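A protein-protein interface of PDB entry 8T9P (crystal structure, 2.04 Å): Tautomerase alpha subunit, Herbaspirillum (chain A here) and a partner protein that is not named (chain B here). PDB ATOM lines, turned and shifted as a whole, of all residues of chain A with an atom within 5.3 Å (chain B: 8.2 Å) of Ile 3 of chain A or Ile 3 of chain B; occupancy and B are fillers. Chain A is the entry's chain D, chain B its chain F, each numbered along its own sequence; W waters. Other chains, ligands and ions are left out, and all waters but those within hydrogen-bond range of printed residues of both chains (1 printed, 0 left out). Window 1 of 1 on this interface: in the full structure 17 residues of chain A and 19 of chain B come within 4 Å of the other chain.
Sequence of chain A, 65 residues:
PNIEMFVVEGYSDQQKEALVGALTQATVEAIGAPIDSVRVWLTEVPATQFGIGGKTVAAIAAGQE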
ATOM      1  N   PRO A   1      -0.388 -21.711  39.296  1.00  0.00           N
ATOM      2  CA  PRO A   1       0.528 -21.952  38.169  1.00  0.00           C
ATOM      3  C   PRO A   1       0.558 -20.760  37.225  1.00  0.00           C
ATOM      4  O   PRO A   1      -0.501 -20.204  36.900  1.00  0.00           O
ATOM      5  CB  PRO A   1      -0.063 -23.187  37.480  1.00  0.00           C
ATOM      6  CG  PRO A   1      -1.103 -23.737  38.440  1.00  0.00           C
ATOM      7  CD  PRO A   1      -1.593 -22.556  39.205  1.00  0.00           C
ATOM      8  N   ASN A   2       1.762 -20.351  36.824  1.00  0.00           N
ATOM      9  CA  ASN A   2       1.957 -19.354  35.781  1.00  0.00           C
ATOM     10  C   ASN A   2       2.630 -20.003  34.584  1.00  0.00           C
ATOM     11  O   ASN A   2       3.679 -20.642  34.728  1.00  0.00           O
ATOM     12  CB  ASN A   2       2.801 -18.196  36.301  1.00  0.00           C
ATOM     13  CG  ASN A   2       2.297 -17.703  37.659  1.00  0.00           C
ATOM     14  OD1 ASN A   2       1.274 -17.024  37.724  1.00  0.00           O
ATOM     15  ND2 ASN A   2       2.950 -18.126  38.734  1.00  0.00           N
ATOM     16  N   ILE A   3       2.042 -19.822  33.406  1.00  0.00           N
ATOM     17  CA  ILE A   3       2.568 -20.403  32.169  1.00  0.00           C
ATOM     18  C   ILE A   3       2.844 -19.255  31.214  1.00  0.00           C
ATOM     19  O   ILE A   3       1.922 -18.534  30.807  1.00  0.00           O
ATOM     20  CB  ILE A   3       1.607 -21.432  31.566  1.00  0.00           C
ATOM     21  CG1 ILE A   3       1.395 -22.554  32.574  1.00  0.00           C
ATOM     22  CG2 ILE A   3       2.167 -22.043  30.256  1.00  0.00           C
ATOM     23  CD1 ILE A   3       0.022 -23.012  32.649  1.00  0.00           C
ATOM     24  N   GLU A   4       4.118 -19.050  30.893  1.00  0.00           N
ATOM     25  CA  GLU A   4       4.533 -18.140  29.834  1.00  0.00           C
ATOM     26  C   GLU A   4       5.020 -18.962  28.644  1.00  0.00           C
ATOM     27  O   GLU A   4       5.943 -19.779  28.784  1.00  0.00           O
ATOM     28  CB  GLU A   4       5.633 -17.211  30.322  1.00  0.00           C
ATOM     29  CG  GLU A   4       6.059 -16.174  29.310  1.00  0.00           C
ATOM     30  CD  GLU A   4       7.124 -15.258  29.870  1.00  0.00           C
ATOM     31  OE1 GLU A   4       7.735 -15.611  30.905  1.00  0.00           O
ATOM     32  OE2 GLU A   4       7.353 -14.186  29.275  1.00  0.00           O
ATOM     33  N   MET A   5       4.397 -18.760  27.488  1.00  0.00           N
ATOM     34  CA  MET A   5       4.819 -19.409  26.248  1.00  0.00           C
ATOM     35  C   MET A   5       5.360 -18.388  25.265  1.00  0.00           C
ATOM     36  O   MET A   5       4.633 -17.487  24.828  1.00  0.00           O
ATOM     37  CB  MET A   5       3.688 -20.178  25.575  1.00  0.00           C
ATOM     38  CG  MET A   5       4.253 -21.000  24.401  1.00  0.00           C
ATOM     39  SD  MET A   5       3.027 -22.118  23.741  1.00  0.00           S
ATOM     40  CE  MET A   5       3.867 -22.789  22.333  1.00  0.00           C
ATOM     41  N   PHE A   6       6.611 -18.569  24.872  1.00  0.00           N
ATOM     42  CA  PHE A   6       7.219 -17.748  23.838  1.00  0.00           C
ATOM     43  C   PHE A   6       6.865 -18.315  22.474  1.00  0.00           C
ATOM     44  O   PHE A   6       7.162 -19.477  22.192  1.00  0.00           O
ATOM     45  CB  PHE A   6       8.731 -17.700  24.037  1.00  0.00           C
ATOM     46  CG  PHE A   6       9.134 -17.118  25.365  1.00  0.00           C
ATOM     47  CD1 PHE A   6       9.099 -17.896  26.521  1.00  0.00           C
ATOM     48  CD2 PHE A   6       9.524 -15.799  25.466  1.00  0.00           C
ATOM     49  CE1 PHE A   6       9.448 -17.375  27.759  1.00  0.00           C
ATOM     50  CE2 PHE A   6       9.879 -15.260  26.716  1.00  0.00           C
ATOM     51  CZ  PHE A   6       9.847 -16.053  27.852  1.00  0.00           C
ATOM     52  N   LEU A  23      -3.533 -24.565  26.798  1.00  0.00           N
ATOM     53  CA  LEU A  23      -2.513 -24.592  27.838  1.00  0.00           C
ATOM     54  C   LEU A  23      -3.139 -24.597  29.227  1.00  0.00           C
ATOM     55  O   LEU A  23      -2.683 -25.321  30.121  1.00  0.00           O
ATOM     56  CB  LEU A  23      -1.565 -23.397  27.685  1.00  0.00           C
ATOM     57  CG  LEU A  23      -0.603 -23.432  26.488  1.00  0.00           C
ATOM     58  CD1 LEU A  23       0.168 -22.121  26.373  1.00  0.00           C
ATOM     59  CD2 LEU A  23       0.356 -24.627  26.539  1.00  0.00           C
ATOM     60  N   THR A  27      -3.031 -27.803  32.053  1.00  0.00           N
ATOM     61  CA  THR A  27      -2.564 -27.651  33.424  1.00  0.00           C
ATOM     62  C   THR A  27      -3.595 -28.186  34.414  1.00  0.00           C
ATOM     63  O   THR A  27      -3.263 -28.963  35.320  1.00  0.00           O
ATOM     64  CB  THR A  27      -2.272 -26.178  33.690  1.00  0.00           C
ATOM     65  OG1 THR A  27      -1.298 -25.726  32.744  1.00  0.00           O
ATOM     66  CG2 THR A  27      -1.754 -25.947  35.130  1.00  0.00           C
ATOM     67  N   VAL A  38      -5.044 -20.586  37.289  1.00  0.00           N
ATOM     68  CA  VAL A  38      -4.047 -20.732  36.228  1.00  0.00           C
ATOM     69  C   VAL A  38      -3.937 -19.425  35.458  1.00  0.00           C
ATOM     70  O   VAL A  38      -4.934 -18.901  34.942  1.00  0.00           O
ATOM     71  CB  VAL A  38      -4.417 -21.892  35.285  1.00  0.00           C
ATOM     72  CG1 VAL A  38      -3.343 -22.084  34.170  1.00  0.00           C
ATOM     73  CG2 VAL A  38      -4.630 -23.171  36.084  1.00  0.00           C
ATOM     74  N   ARG A  39      -2.722 -18.907  35.349  1.00  0.00           N
ATOM     75  CA  ARG A  39      -2.441 -17.768  34.493  1.00  0.00           C
ATOM     76  C   ARG A  39      -1.568 -18.236  33.341  1.00  0.00           C
ATOM     77  O   ARG A  39      -0.530 -18.870  33.553  1.00  0.00           O
ATOM     78  CB  ARG A  39      -1.771 -16.638  35.275  1.00  0.00           C
ATOM     79  CG  ARG A  39      -2.737 -16.019  36.272  1.00  0.00           C
ATOM     80  CD  ARG A  39      -2.192 -14.796  36.966  1.00  0.00           C
ATOM     81  NE  ARG A  39      -2.792 -14.680  38.295  1.00  0.00           N
ATOM     82  CZ  ARG A  39      -2.878 -13.555  39.001  1.00  0.00           C
ATOM     83  NH1 ARG A  39      -2.422 -12.413  38.501  1.00  0.00           N
ATOM     84  NH2 ARG A  39      -3.445 -13.574  40.204  1.00  0.00           N
ATOM     85  N   VAL A  40      -2.008 -17.946  32.127  1.00  0.00           N
ATOM     86  CA  VAL A  40      -1.285 -18.294  30.916  1.00  0.00           C
ATOM     87  C   VAL A  40      -1.136 -17.023  30.108  1.00  0.00           C
ATOM     88  O   VAL A  40      -2.128 -16.329  29.858  1.00  0.00           O
ATOM     89  CB  VAL A  40      -2.023 -19.371  30.094  1.00  0.00           C
ATOM     90  CG1 VAL A  40      -1.324 -19.601  28.742  1.00  0.00           C
ATOM     91  CG2 VAL A  40      -2.131 -20.668  30.889  1.00  0.00           C
ATOM     92  N   TRP A  41       0.093 -16.701  29.717  1.00  0.00           N
ATOM     93  CA  TRP A  41       0.258 -15.618  28.765  1.00  0.00           C
ATOM     94  C   TRP A  41       1.276 -16.001  27.705  1.00  0.00           C
ATOM     95  O   TRP A  41       2.145 -16.855  27.912  1.00  0.00           O
ATOM     96  CB  TRP A  41       0.642 -14.300  29.434  1.00  0.00           C
ATOM     97  CG  TRP A  41       1.944 -14.277  30.125  1.00  0.00           C
ATOM     98  CD1 TRP A  41       3.087 -13.703  29.677  1.00  0.00           C
ATOM     99  CD2 TRP A  41       2.236 -14.804  31.427  1.00  0.00           C
ATOM    100  NE1 TRP A  41       4.082 -13.851  30.612  1.00  0.00           N
ATOM    101  CE2 TRP A  41       3.590 -14.538  31.688  1.00  0.00           C
ATOM    102  CE3 TRP A  41       1.488 -15.496  32.387  1.00  0.00           C
ATOM    103  CZ2 TRP A  41       4.215 -14.927  32.871  1.00  0.00           C
ATOM    104  CZ3 TRP A  41       2.107 -15.883  33.558  1.00  0.00           C
ATOM    105  CH2 TRP A  41       3.462 -15.601  33.790  1.00  0.00           C
ATOM    106  N   SER B   1       9.033 -23.876  19.970  1.00  0.00           N
ATOM    107  CA  SER B   1       8.682 -22.854  20.967  1.00  0.00           C
ATOM    108  C   SER B   1       8.680 -23.349  22.409  1.00  0.00           C
ATOM    109  O   SER B   1       8.674 -24.550  22.695  1.00  0.00           O
ATOM    110  CB  SER B   1       7.333 -22.290  20.693  1.00  0.00           C
ATOM    111  OG  SER B   1       6.425 -23.278  21.099  1.00  0.00           O
ATOM    112  N   ILE B   2       8.655 -22.383  23.317  1.00  0.00           N
ATOM    113  CA  ILE B   2       9.249 -22.543  24.633  1.00  0.00           C
ATOM    114  C   ILE B   2       8.217 -22.160  25.677  1.00  0.00           C
ATOM    115  O   ILE B   2       7.669 -21.052  25.646  1.00  0.00           O
ATOM    116  CB  ILE B   2      10.539 -21.704  24.746  1.00  0.00           C
ATOM    117  CG1 ILE B   2      11.525 -22.214  23.673  1.00  0.00           C
ATOM    118  CG2 ILE B   2      11.142 -21.810  26.155  1.00  0.00           C
ATOM    119  CD1 ILE B   2      12.652 -21.275  23.334  1.00  0.00           C
ATOM    120  N   ILE B   3       7.930 -23.086  26.579  1.00  0.00           N
ATOM    121  CA  ILE B   3       6.891 -22.928  27.586  1.00  0.00           C
ATOM    122  C   ILE B   3       7.572 -22.927  28.946  1.00  0.00           C
ATOM    123  O   ILE B   3       8.206 -23.922  29.323  1.00  0.00           O
ATOM    124  CB  ILE B   3       5.853 -24.055  27.496  1.00  0.00           C
ATOM    125  CG1 ILE B   3       5.237 -24.110  26.090  1.00  0.00           C
ATOM    126  CG2 ILE B   3       4.770 -23.865  28.546  1.00  0.00           C
ATOM    127  CD1 ILE B   3       4.401 -25.386  25.833  1.00  0.00           C
ATOM    128  N   GLN B   4       7.467 -21.815  29.669  1.00  0.00           N
ATOM    129  CA  GLN B   4       8.044 -21.706  31.001  1.00  0.00           C
ATOM    130  C   GLN B   4       6.937 -21.689  32.039  1.00  0.00           C
ATOM    131  O   GLN B   4       6.021 -20.870  31.953  1.00  0.00           O
ATOM    132  CB  GLN B   4       8.918 -20.452  31.116  1.00  0.00           C
ATOM    133  CG  GLN B   4      10.280 -20.771  30.531  1.00  0.00           C
ATOM    134  CD  GLN B   4      11.128 -19.582  30.221  1.00  0.00           C
ATOM    135  OE1 GLN B   4      12.029 -19.678  29.386  1.00  0.00           O
ATOM    136  NE2 GLN B   4      10.889 -18.462  30.910  1.00  0.00           N
ATOM    137  N   VAL B   5       7.028 -22.596  33.011  1.00  0.00           N
ATOM    138  CA  VAL B   5       6.023 -22.747  34.058  1.00  0.00           C
ATOM    139  C   VAL B   5       6.651 -22.424  35.412  1.00  0.00           C
ATOM    140  O   VAL B   5       7.726 -22.942  35.741  1.00  0.00           O
ATOM    141  CB  VAL B   5       5.443 -24.170  34.078  1.00  0.00           C
ATOM    142  CG1 VAL B   5       4.320 -24.273  35.113  1.00  0.00           C
ATOM    143  CG2 VAL B   5       4.958 -24.589  32.663  1.00  0.00           C
ATOM    144  N   THR B   6       5.973 -21.583  36.199  1.00  0.00           N
ATOM    145  CA  THR B   6       6.274 -21.414  37.615  1.00  0.00           C
ATOM    146  C   THR B   6       5.047 -21.810  38.432  1.00  0.00           C
ATOM    147  O   THR B   6       3.908 -21.507  38.057  1.00  0.00           O
ATOM    148  CB  THR B   6       6.683 -19.975  37.965  1.00  0.00           C
ATOM    149  OG1 THR B   6       5.579 -19.099  37.734  1.00  0.00           O
ATOM    150  CG2 THR B   6       7.859 -19.518  37.123  1.00  0.00           C
ATOM    151  N   PHE B   7       5.282 -22.502  39.538  1.00  0.00           N
ATOM    152  CA  PHE B   7       4.188 -22.983  40.370  1.00  0.00           C
ATOM    153  C   PHE B   7       4.774 -23.317  41.736  1.00  0.00           C
ATOM    154  O   PHE B   7       5.984 -23.520  41.877  1.00  0.00           O
ATOM    155  CB  PHE B   7       3.498 -24.152  39.655  1.00  0.00           C
ATOM    156  CG  PHE B   7       4.341 -25.387  39.509  1.00  0.00           C
ATOM    157  CD1 PHE B   7       5.485 -25.382  38.738  1.00  0.00           C
ATOM    158  CD2 PHE B   7       3.795 -26.611  39.809  1.00  0.00           C
ATOM    159  CE1 PHE B   7       6.226 -26.544  38.537  1.00  0.00           C
ATOM    160  CE2 PHE B   7       4.500 -27.782  39.563  1.00  0.00           C
ATOM    161  CZ  PHE B   7       5.718 -27.743  38.930  1.00  0.00           C
ATOM    162  N   LEU B  19       2.426 -32.913  33.286  1.00  0.00           N
ATOM    163  CA  LEU B  19       2.283 -31.532  32.853  1.00  0.00           C
ATOM    164  C   LEU B  19       3.136 -31.244  31.624  1.00  0.00           C
ATOM    165  O   LEU B  19       2.708 -30.519  30.722  1.00  0.00           O
ATOM    166  CB  LEU B  19       2.667 -30.601  34.010  1.00  0.00           C
ATOM    167  CG  LEU B  19       2.508 -29.113  33.724  1.00  0.00           C
ATOM    168  CD1 LEU B  19       1.045 -28.857  33.380  1.00  0.00           C
ATOM    169  CD2 LEU B  19       2.979 -28.282  34.931  1.00  0.00           C
ATOM    170  N   ILE B  20       4.350 -31.792  31.575  1.00  0.00           N
ATOM    171  CA  ILE B  20       5.206 -31.587  30.409  1.00  0.00           C
ATOM    172  C   ILE B  20       4.598 -32.240  29.171  1.00  0.00           C
ATOM    173  O   ILE B  20       4.588 -31.651  28.083  1.00  0.00           O
ATOM    174  CB  ILE B  20       6.629 -32.110  30.688  1.00  0.00           C
ATOM    175  CG1 ILE B  20       7.411 -31.071  31.525  1.00  0.00           C
ATOM    176  CG2 ILE B  20       7.350 -32.382  29.372  1.00  0.00           C
ATOM    177  CD1 ILE B  20       8.619 -31.653  32.270  1.00  0.00           C
ATOM    178  N   ALA B  21       4.064 -33.457  29.316  1.00  0.00           N
ATOM    179  CA  ALA B  21       3.394 -34.099  28.188  1.00  0.00           C
ATOM    180  C   ALA B  21       2.155 -33.315  27.758  1.00  0.00           C
ATOM    181  O   ALA B  21       1.920 -33.104  26.563  1.00  0.00           O
ATOM    182  CB  ALA B  21       3.029 -35.544  28.554  1.00  0.00           C
ATOM    183  N   ALA B  22       1.354 -32.872  28.715  1.00  0.00           N
ATOM    184  CA  ALA B  22       0.085 -32.233  28.380  1.00  0.00           C
ATOM    185  C   ALA B  22       0.292 -30.850  27.770  1.00  0.00           C
ATOM    186  O   ALA B  22      -0.439 -30.467  26.849  1.00  0.00           O
ATOM    187  CB  ALA B  22      -0.803 -32.151  29.621  1.00  0.00           C
ATOM    188  N   LEU B  23       1.283 -30.087  28.263  1.00  0.00           N
ATOM    189  CA  LEU B  23       1.576 -28.782  27.668  1.00  0.00           C
ATOM    190  C   LEU B  23       2.115 -28.933  26.253  1.00  0.00           C
ATOM    191  O   LEU B  23       1.772 -28.148  25.355  1.00  0.00           O
ATOM    192  CB  LEU B  23       2.576 -28.003  28.544  1.00  0.00           C
ATOM    193  CG  LEU B  23       1.965 -27.538  29.880  1.00  0.00           C
ATOM    194  CD1 LEU B  23       3.018 -26.917  30.841  1.00  0.00           C
ATOM    195  CD2 LEU B  23       0.857 -26.523  29.635  1.00  0.00           C
ATOM    196  N   THR B  24       2.958 -29.935  26.040  1.00  0.00           N
ATOM    197  CA  THR B  24       3.491 -30.195  24.709  1.00  0.00           C
ATOM    198  C   THR B  24       2.382 -30.597  23.741  1.00  0.00           C
ATOM    199  O   THR B  24       2.263 -30.024  22.650  1.00  0.00           O
ATOM    200  CB  THR B  24       4.574 -31.267  24.798  1.00  0.00           C
ATOM    201  OG1 THR B  24       5.621 -30.788  25.666  1.00  0.00           O
ATOM    202  CG2 THR B  24       5.157 -31.556  23.415  1.00  0.00           C
ATOM    203  N   ASP B  25       1.545 -31.571  24.137  1.00  0.00           N
ATOM    204  CA  ASP B  25       0.387 -31.962  23.329  1.00  0.00           C
ATOM    205  C   ASP B  25      -0.475 -30.761  22.974  1.00  0.00           C
ATOM    206  O   ASP B  25      -0.996 -30.669  21.854  1.00  0.00           O
ATOM    207  CB  ASP B  25      -0.487 -32.981  24.078  1.00  0.00           C
ATOM    208  CG  ASP B  25       0.127 -34.362  24.147  1.00  0.00           C
ATOM    209  OD1 ASP B  25       1.193 -34.593  23.523  1.00  0.00           O
ATOM    210  OD2 ASP B  25      -0.454 -35.218  24.866  1.00  0.00           O
ATOM    211  N   ALA B  26      -0.661 -29.846  23.931  1.00  0.00           N
ATOM    212  CA  ALA B  26      -1.517 -28.683  23.714  1.00  0.00           C
ATOM    213  C   ALA B  26      -0.950 -27.759  22.650  1.00  0.00           C
ATOM    214  O   ALA B  26      -1.708 -27.185  21.864  1.00  0.00           O
ATOM    215  CB  ALA B  26      -1.697 -27.897  25.017  1.00  0.00           C
ATOM    216  N   ALA B  27       0.372 -27.534  22.670  1.00  0.00           N
ATOM    217  CA  ALA B  27       1.007 -26.695  21.658  1.00  0.00           C
ATOM    218  C   ALA B  27       0.963 -27.365  20.290  1.00  0.00           C
ATOM    219  O   ALA B  27       0.655 -26.713  19.287  1.00  0.00           O
ATOM    220  CB  ALA B  27       2.458 -26.384  22.050  1.00  0.00           C
ATOM    221  N   VAL B  28       1.265 -28.665  20.232  1.00  0.00           N
ATOM    222  CA  VAL B  28       1.269 -29.372  18.954  1.00  0.00           C
ATOM    223  C   VAL B  28      -0.136 -29.384  18.353  1.00  0.00           C
ATOM    224  O   VAL B  28      -0.345 -29.045  17.182  1.00  0.00           O
ATOM    225  CB  VAL B  28       1.817 -30.803  19.135  1.00  0.00           C
ATOM    226  CG1 VAL B  28       1.577 -31.590  17.892  1.00  0.00           C
ATOM    227  CG2 VAL B  28       3.340 -30.800  19.484  1.00  0.00           C
ATOM    228  N   ILE B  33       2.711 -26.781  15.952  1.00  0.00           N
ATOM    229  CA  ILE B  33       4.154 -26.750  16.150  1.00  0.00           C
ATOM    230  C   ILE B  33       4.667 -28.181  16.111  1.00  0.00           C
ATOM    231  O   ILE B  33       4.013 -29.103  16.610  1.00  0.00           O
ATOM    232  CB  ILE B  33       4.506 -26.057  17.486  1.00  0.00           C
ATOM    233  CG1 ILE B  33       4.095 -24.593  17.453  1.00  0.00           C
ATOM    234  CG2 ILE B  33       6.007 -26.049  17.720  1.00  0.00           C
ATOM    235  CD1 ILE B  33       4.484 -23.835  18.719  1.00  0.00           C
ATOM    236  N   GLU B  37      10.251 -29.436  18.401  1.00  0.00           N
ATOM    237  CA  GLU B  37      10.604 -28.059  18.682  1.00  0.00           C
ATOM    238  C   GLU B  37      10.118 -27.598  20.044  1.00  0.00           C
ATOM    239  O   GLU B  37      10.602 -26.580  20.536  1.00  0.00           O
ATOM    240  CB  GLU B  37      10.029 -27.132  17.615  1.00  0.00           C
ATOM    241  CG  GLU B  37      10.717 -27.287  16.266  1.00  0.00           C
ATOM    242  CD  GLU B  37      12.215 -26.938  16.350  1.00  0.00           C
ATOM    243  OE1 GLU B  37      12.592 -25.953  17.031  1.00  0.00           O
ATOM    244  OE2 GLU B  37      13.020 -27.658  15.745  1.00  0.00           O
ATOM    245  N   VAL B  38       9.188 -28.318  20.666  1.00  0.00           N
ATOM    246  CA  VAL B  38       8.567 -27.828  21.890  1.00  0.00           C
ATOM    247  C   VAL B  38       9.486 -28.091  23.077  1.00  0.00           C
ATOM    248  O   VAL B  38       9.901 -29.232  23.321  1.00  0.00           O
ATOM    249  CB  VAL B  38       7.196 -28.485  22.113  1.00  0.00           C
ATOM    250  CG1 VAL B  38       6.623 -27.974  23.440  1.00  0.00           C
ATOM    251  CG2 VAL B  38       6.241 -28.143  20.940  1.00  0.00           C
ATOM    252  N   ARG B  39       9.782 -27.038  23.832  1.00  0.00           N
ATOM    253  CA  ARG B  39      10.513 -27.158  25.081  1.00  0.00           C
ATOM    254  C   ARG B  39       9.624 -26.689  26.215  1.00  0.00           C
ATOM    255  O   ARG B  39       8.875 -25.723  26.062  1.00  0.00           O
ATOM    256  CB  ARG B  39      11.814 -26.329  25.055  1.00  0.00           C
ATOM    257  CG  ARG B  39      12.689 -26.590  23.833  1.00  0.00           C
ATOM    258  CD  ARG B  39      13.602 -27.774  24.063  1.00  0.00           C
ATOM    259  NE  ARG B  39      14.541 -28.005  22.948  1.00  0.00           N
ATOM    260  CZ  ARG B  39      14.214 -28.664  21.835  1.00  0.00           C
ATOM    261  NH1 ARG B  39      12.975 -29.133  21.679  1.00  0.00           N
ATOM    262  NH2 ARG B  39      15.118 -28.880  20.895  1.00  0.00           N
ATOM    263  N   VAL B  40       9.720 -27.366  27.358  1.00  0.00           N
ATOM    264  CA  VAL B  40       8.971 -27.002  28.558  1.00  0.00           C
ATOM    265  C   VAL B  40       9.941 -26.932  29.730  1.00  0.00           C
ATOM    266  O   VAL B  40      10.705 -27.876  29.967  1.00  0.00           O
ATOM    267  CB  VAL B  40       7.834 -27.995  28.875  1.00  0.00           C
ATOM    268  CG1 VAL B  40       7.094 -27.562  30.172  1.00  0.00           C
ATOM    269  CG2 VAL B  40       6.823 -28.098  27.716  1.00  0.00           C
ATOM    270  N   ILE B  41       9.893 -25.833  30.474  1.00  0.00           N
ATOM    271  CA  ILE B  41      10.688 -25.682  31.691  1.00  0.00           C
ATOM    272  C   ILE B  41       9.750 -25.493  32.870  1.00  0.00           C
ATOM    273  O   ILE B  41       8.936 -24.563  32.883  1.00  0.00           O
ATOM    274  CB  ILE B  41      11.666 -24.507  31.600  1.00  0.00           C
ATOM    275  CG1 ILE B  41      12.688 -24.752  30.516  1.00  0.00           C
ATOM    276  CG2 ILE B  41      12.400 -24.307  32.957  1.00  0.00           C
ATOM    277  CD1 ILE B  41      13.428 -23.477  30.172  1.00  0.00           C
ATOM    278  N   LEU B  42       9.874 -26.357  33.869  1.00  0.00           N
ATOM    279  CA  LEU B  42       9.116 -26.232  35.109  1.00  0.00           C
ATOM    280  C   LEU B  42      10.062 -25.766  36.208  1.00  0.00           C
ATOM    281  O   LEU B  42      11.123 -26.363  36.404  1.00  0.00           O
ATOM    282  CB  LEU B  42       8.465 -27.555  35.517  1.00  0.00           C
ATOM    283  CG  LEU B  42       7.733 -28.398  34.445  1.00  0.00           C
ATOM    284  CD1 LEU B  42       7.160 -29.670  35.070  1.00  0.00           C
ATOM    285  CD2 LEU B  42       6.607 -27.593  33.823  1.00  0.00           C
ATOM    286  N   LYS B  43       9.669 -24.717  36.923  1.00  0.00           N
ATOM    287  CA  LYS B  43      10.434 -24.191  38.050  1.00  0.00           C
ATOM    288  C   LYS B  43       9.547 -24.218  39.295  1.00  0.00           C
ATOM    289  O   LYS B  43       8.487 -23.582  39.319  1.00  0.00           O
ATOM    290  CB  LYS B  43      10.944 -22.774  37.756  1.00  0.00           C
ATOM    291  CG  LYS B  43      11.565 -22.025  39.006  1.00  0.00           C
ATOM    292  CD  LYS B  43      13.052 -22.352  39.204  1.00  0.00           C
ATOM    293  CE  LYS B  43      13.656 -21.677  40.449  1.00  0.00           C
ATOM    294  NZ  LYS B  43      13.454 -22.523  41.683  1.00  0.00           N
HETATM  295  O   HOH W   1       6.424 -18.800  34.032  1.00  0.00           O
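The backbone carbonyl oxygen of Ile 2 of chain B lies within hydrogen-bond range of the backbone NH of Phe 6 of chain A, 2.8 Å away.
N of Gln 4 of chain B lies within hydrogen-bond range of O of Glu 4 of chain A.
The backbone carbonyl oxygen (O) of Thr 6 of chain B lies within hydrogen-bond range of the backbone NH (N) of Asn 2 of chain A, 2.7 Å away.
O of Pro 1 of chain A is in hydrogen-bond range of N of Arg 39 of chain A (3.0 Å).
The backbone carbonyl oxygen of Arg 39 of chain B lies within hydrogen-bond range of the backbone NH of Ile 3 of chain B (2.8 Å).
The backbone carbonyl oxygen (O) of Val 5 of chain B lies within hydrogen-bond range of the backbone NH (N) of Lys 43 of chain B, at 2.9 Å.
OG1 of Thr 27 of chain A lies within hydrogen-bond range of O of Leu 23 of chain A, at 3.0 Å.
The backbone NH (N) of Val 5 of chain B is in hydrogen-bond range of the backbone carbonyl oxygen (O) of Ile 41 of chain B (2.7 Å).
O of Lys 43 of chain B sits at hydrogen-bond distance from N of Phe 7 of chain B (3.4 Å).
Among the printed residues, merely in contact across the chains: Pro 1 of chain A with Thr 6 of chain B, Pro 1 of chain A with Phe 7 of chain B, Asn 2 of chain A with Gln 4 of chain B, Asn 2 of chain A with Val 5 of chain B, Ile 3 of chain A with Ile 3 of chain B, Ile 3 of chain A with Gln 4 of chain B, Glu 4 of chain A with Ile 2 of chain B, Glu 4 of chain A with Ile 3 of chain B, Met 5 of chain A with Ser 1 of chain B, Met 5 of chain A with Ile 2 of chain B, Met 5 of chain A with Ile 3 of chain B, Met 5 of chain A with Ala 27 of chain B, Met 5 of chain A with Ile 33 of chain B, Phe 6 of chain A with Ser 1 of chain B, Phe 6 of chain A with Gln 4 of chain B, Leu 23 of chain A with Leu 23 of chain B, Thr 27 of chain A with Leu 19 of chain B and Thr 27 of chain A with Leu 23 of chain B.
Ile 3 of chain A touches two residues of chain B.
Of chain A, only Ile 3 (3.6 Å), Glu 4 (3.5 Å) and Met 5 (3.7 Å) come within 4 Å of Ile 3 of chain B.
Of the printed residues of chain A, Ile 33 of chain B touches Met 5 (3.8 Å).
Of the printed residues of chain A, Leu 19 of chain B touches Thr 27 (3.8 Å).
Printed residues of chain A within 4 Å of Thr 6 of chain B: Pro 1 and Asn 2.
Val 40 of chain B touches none of the printed residues of chain A.
Ala 21 of chain B touches none of the printed residues of chain A.
The nearest printed residue of chain A that does not touch Val 5 of chain B is Ile 3 of chain A (4.1 Å).
Of the 12 printed residues of chain A, 8 touch a printed residue of chain B.
Hydrophobic or aromatic side chains of chain A within 4 Å of the printed part of chain B: Ile 3, Met 5, Phe 6 and Leu 23.
Hydrophobic or aromatic side chains of chain B within 4 Å of the printed part of chain A: Ile 3, Val 5, Phe 7, Leu 19, Leu 23, Ala 27 and Ile 33.
Among the printed residues, 21 pairs touch across the chains.
Among the printed residues, no Asp or Glu carboxylate lies within 4 Å of a Lys or Arg side-chain nitrogen of the other chain.
Water W1 lies within hydrogen-bond range of the backbone carbonyl oxygen (O) of Gln 4 of chain B (3.0 Å) and the backbone carbonyl oxygen (O) of Asn 2 of chain A (3.4 Å).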
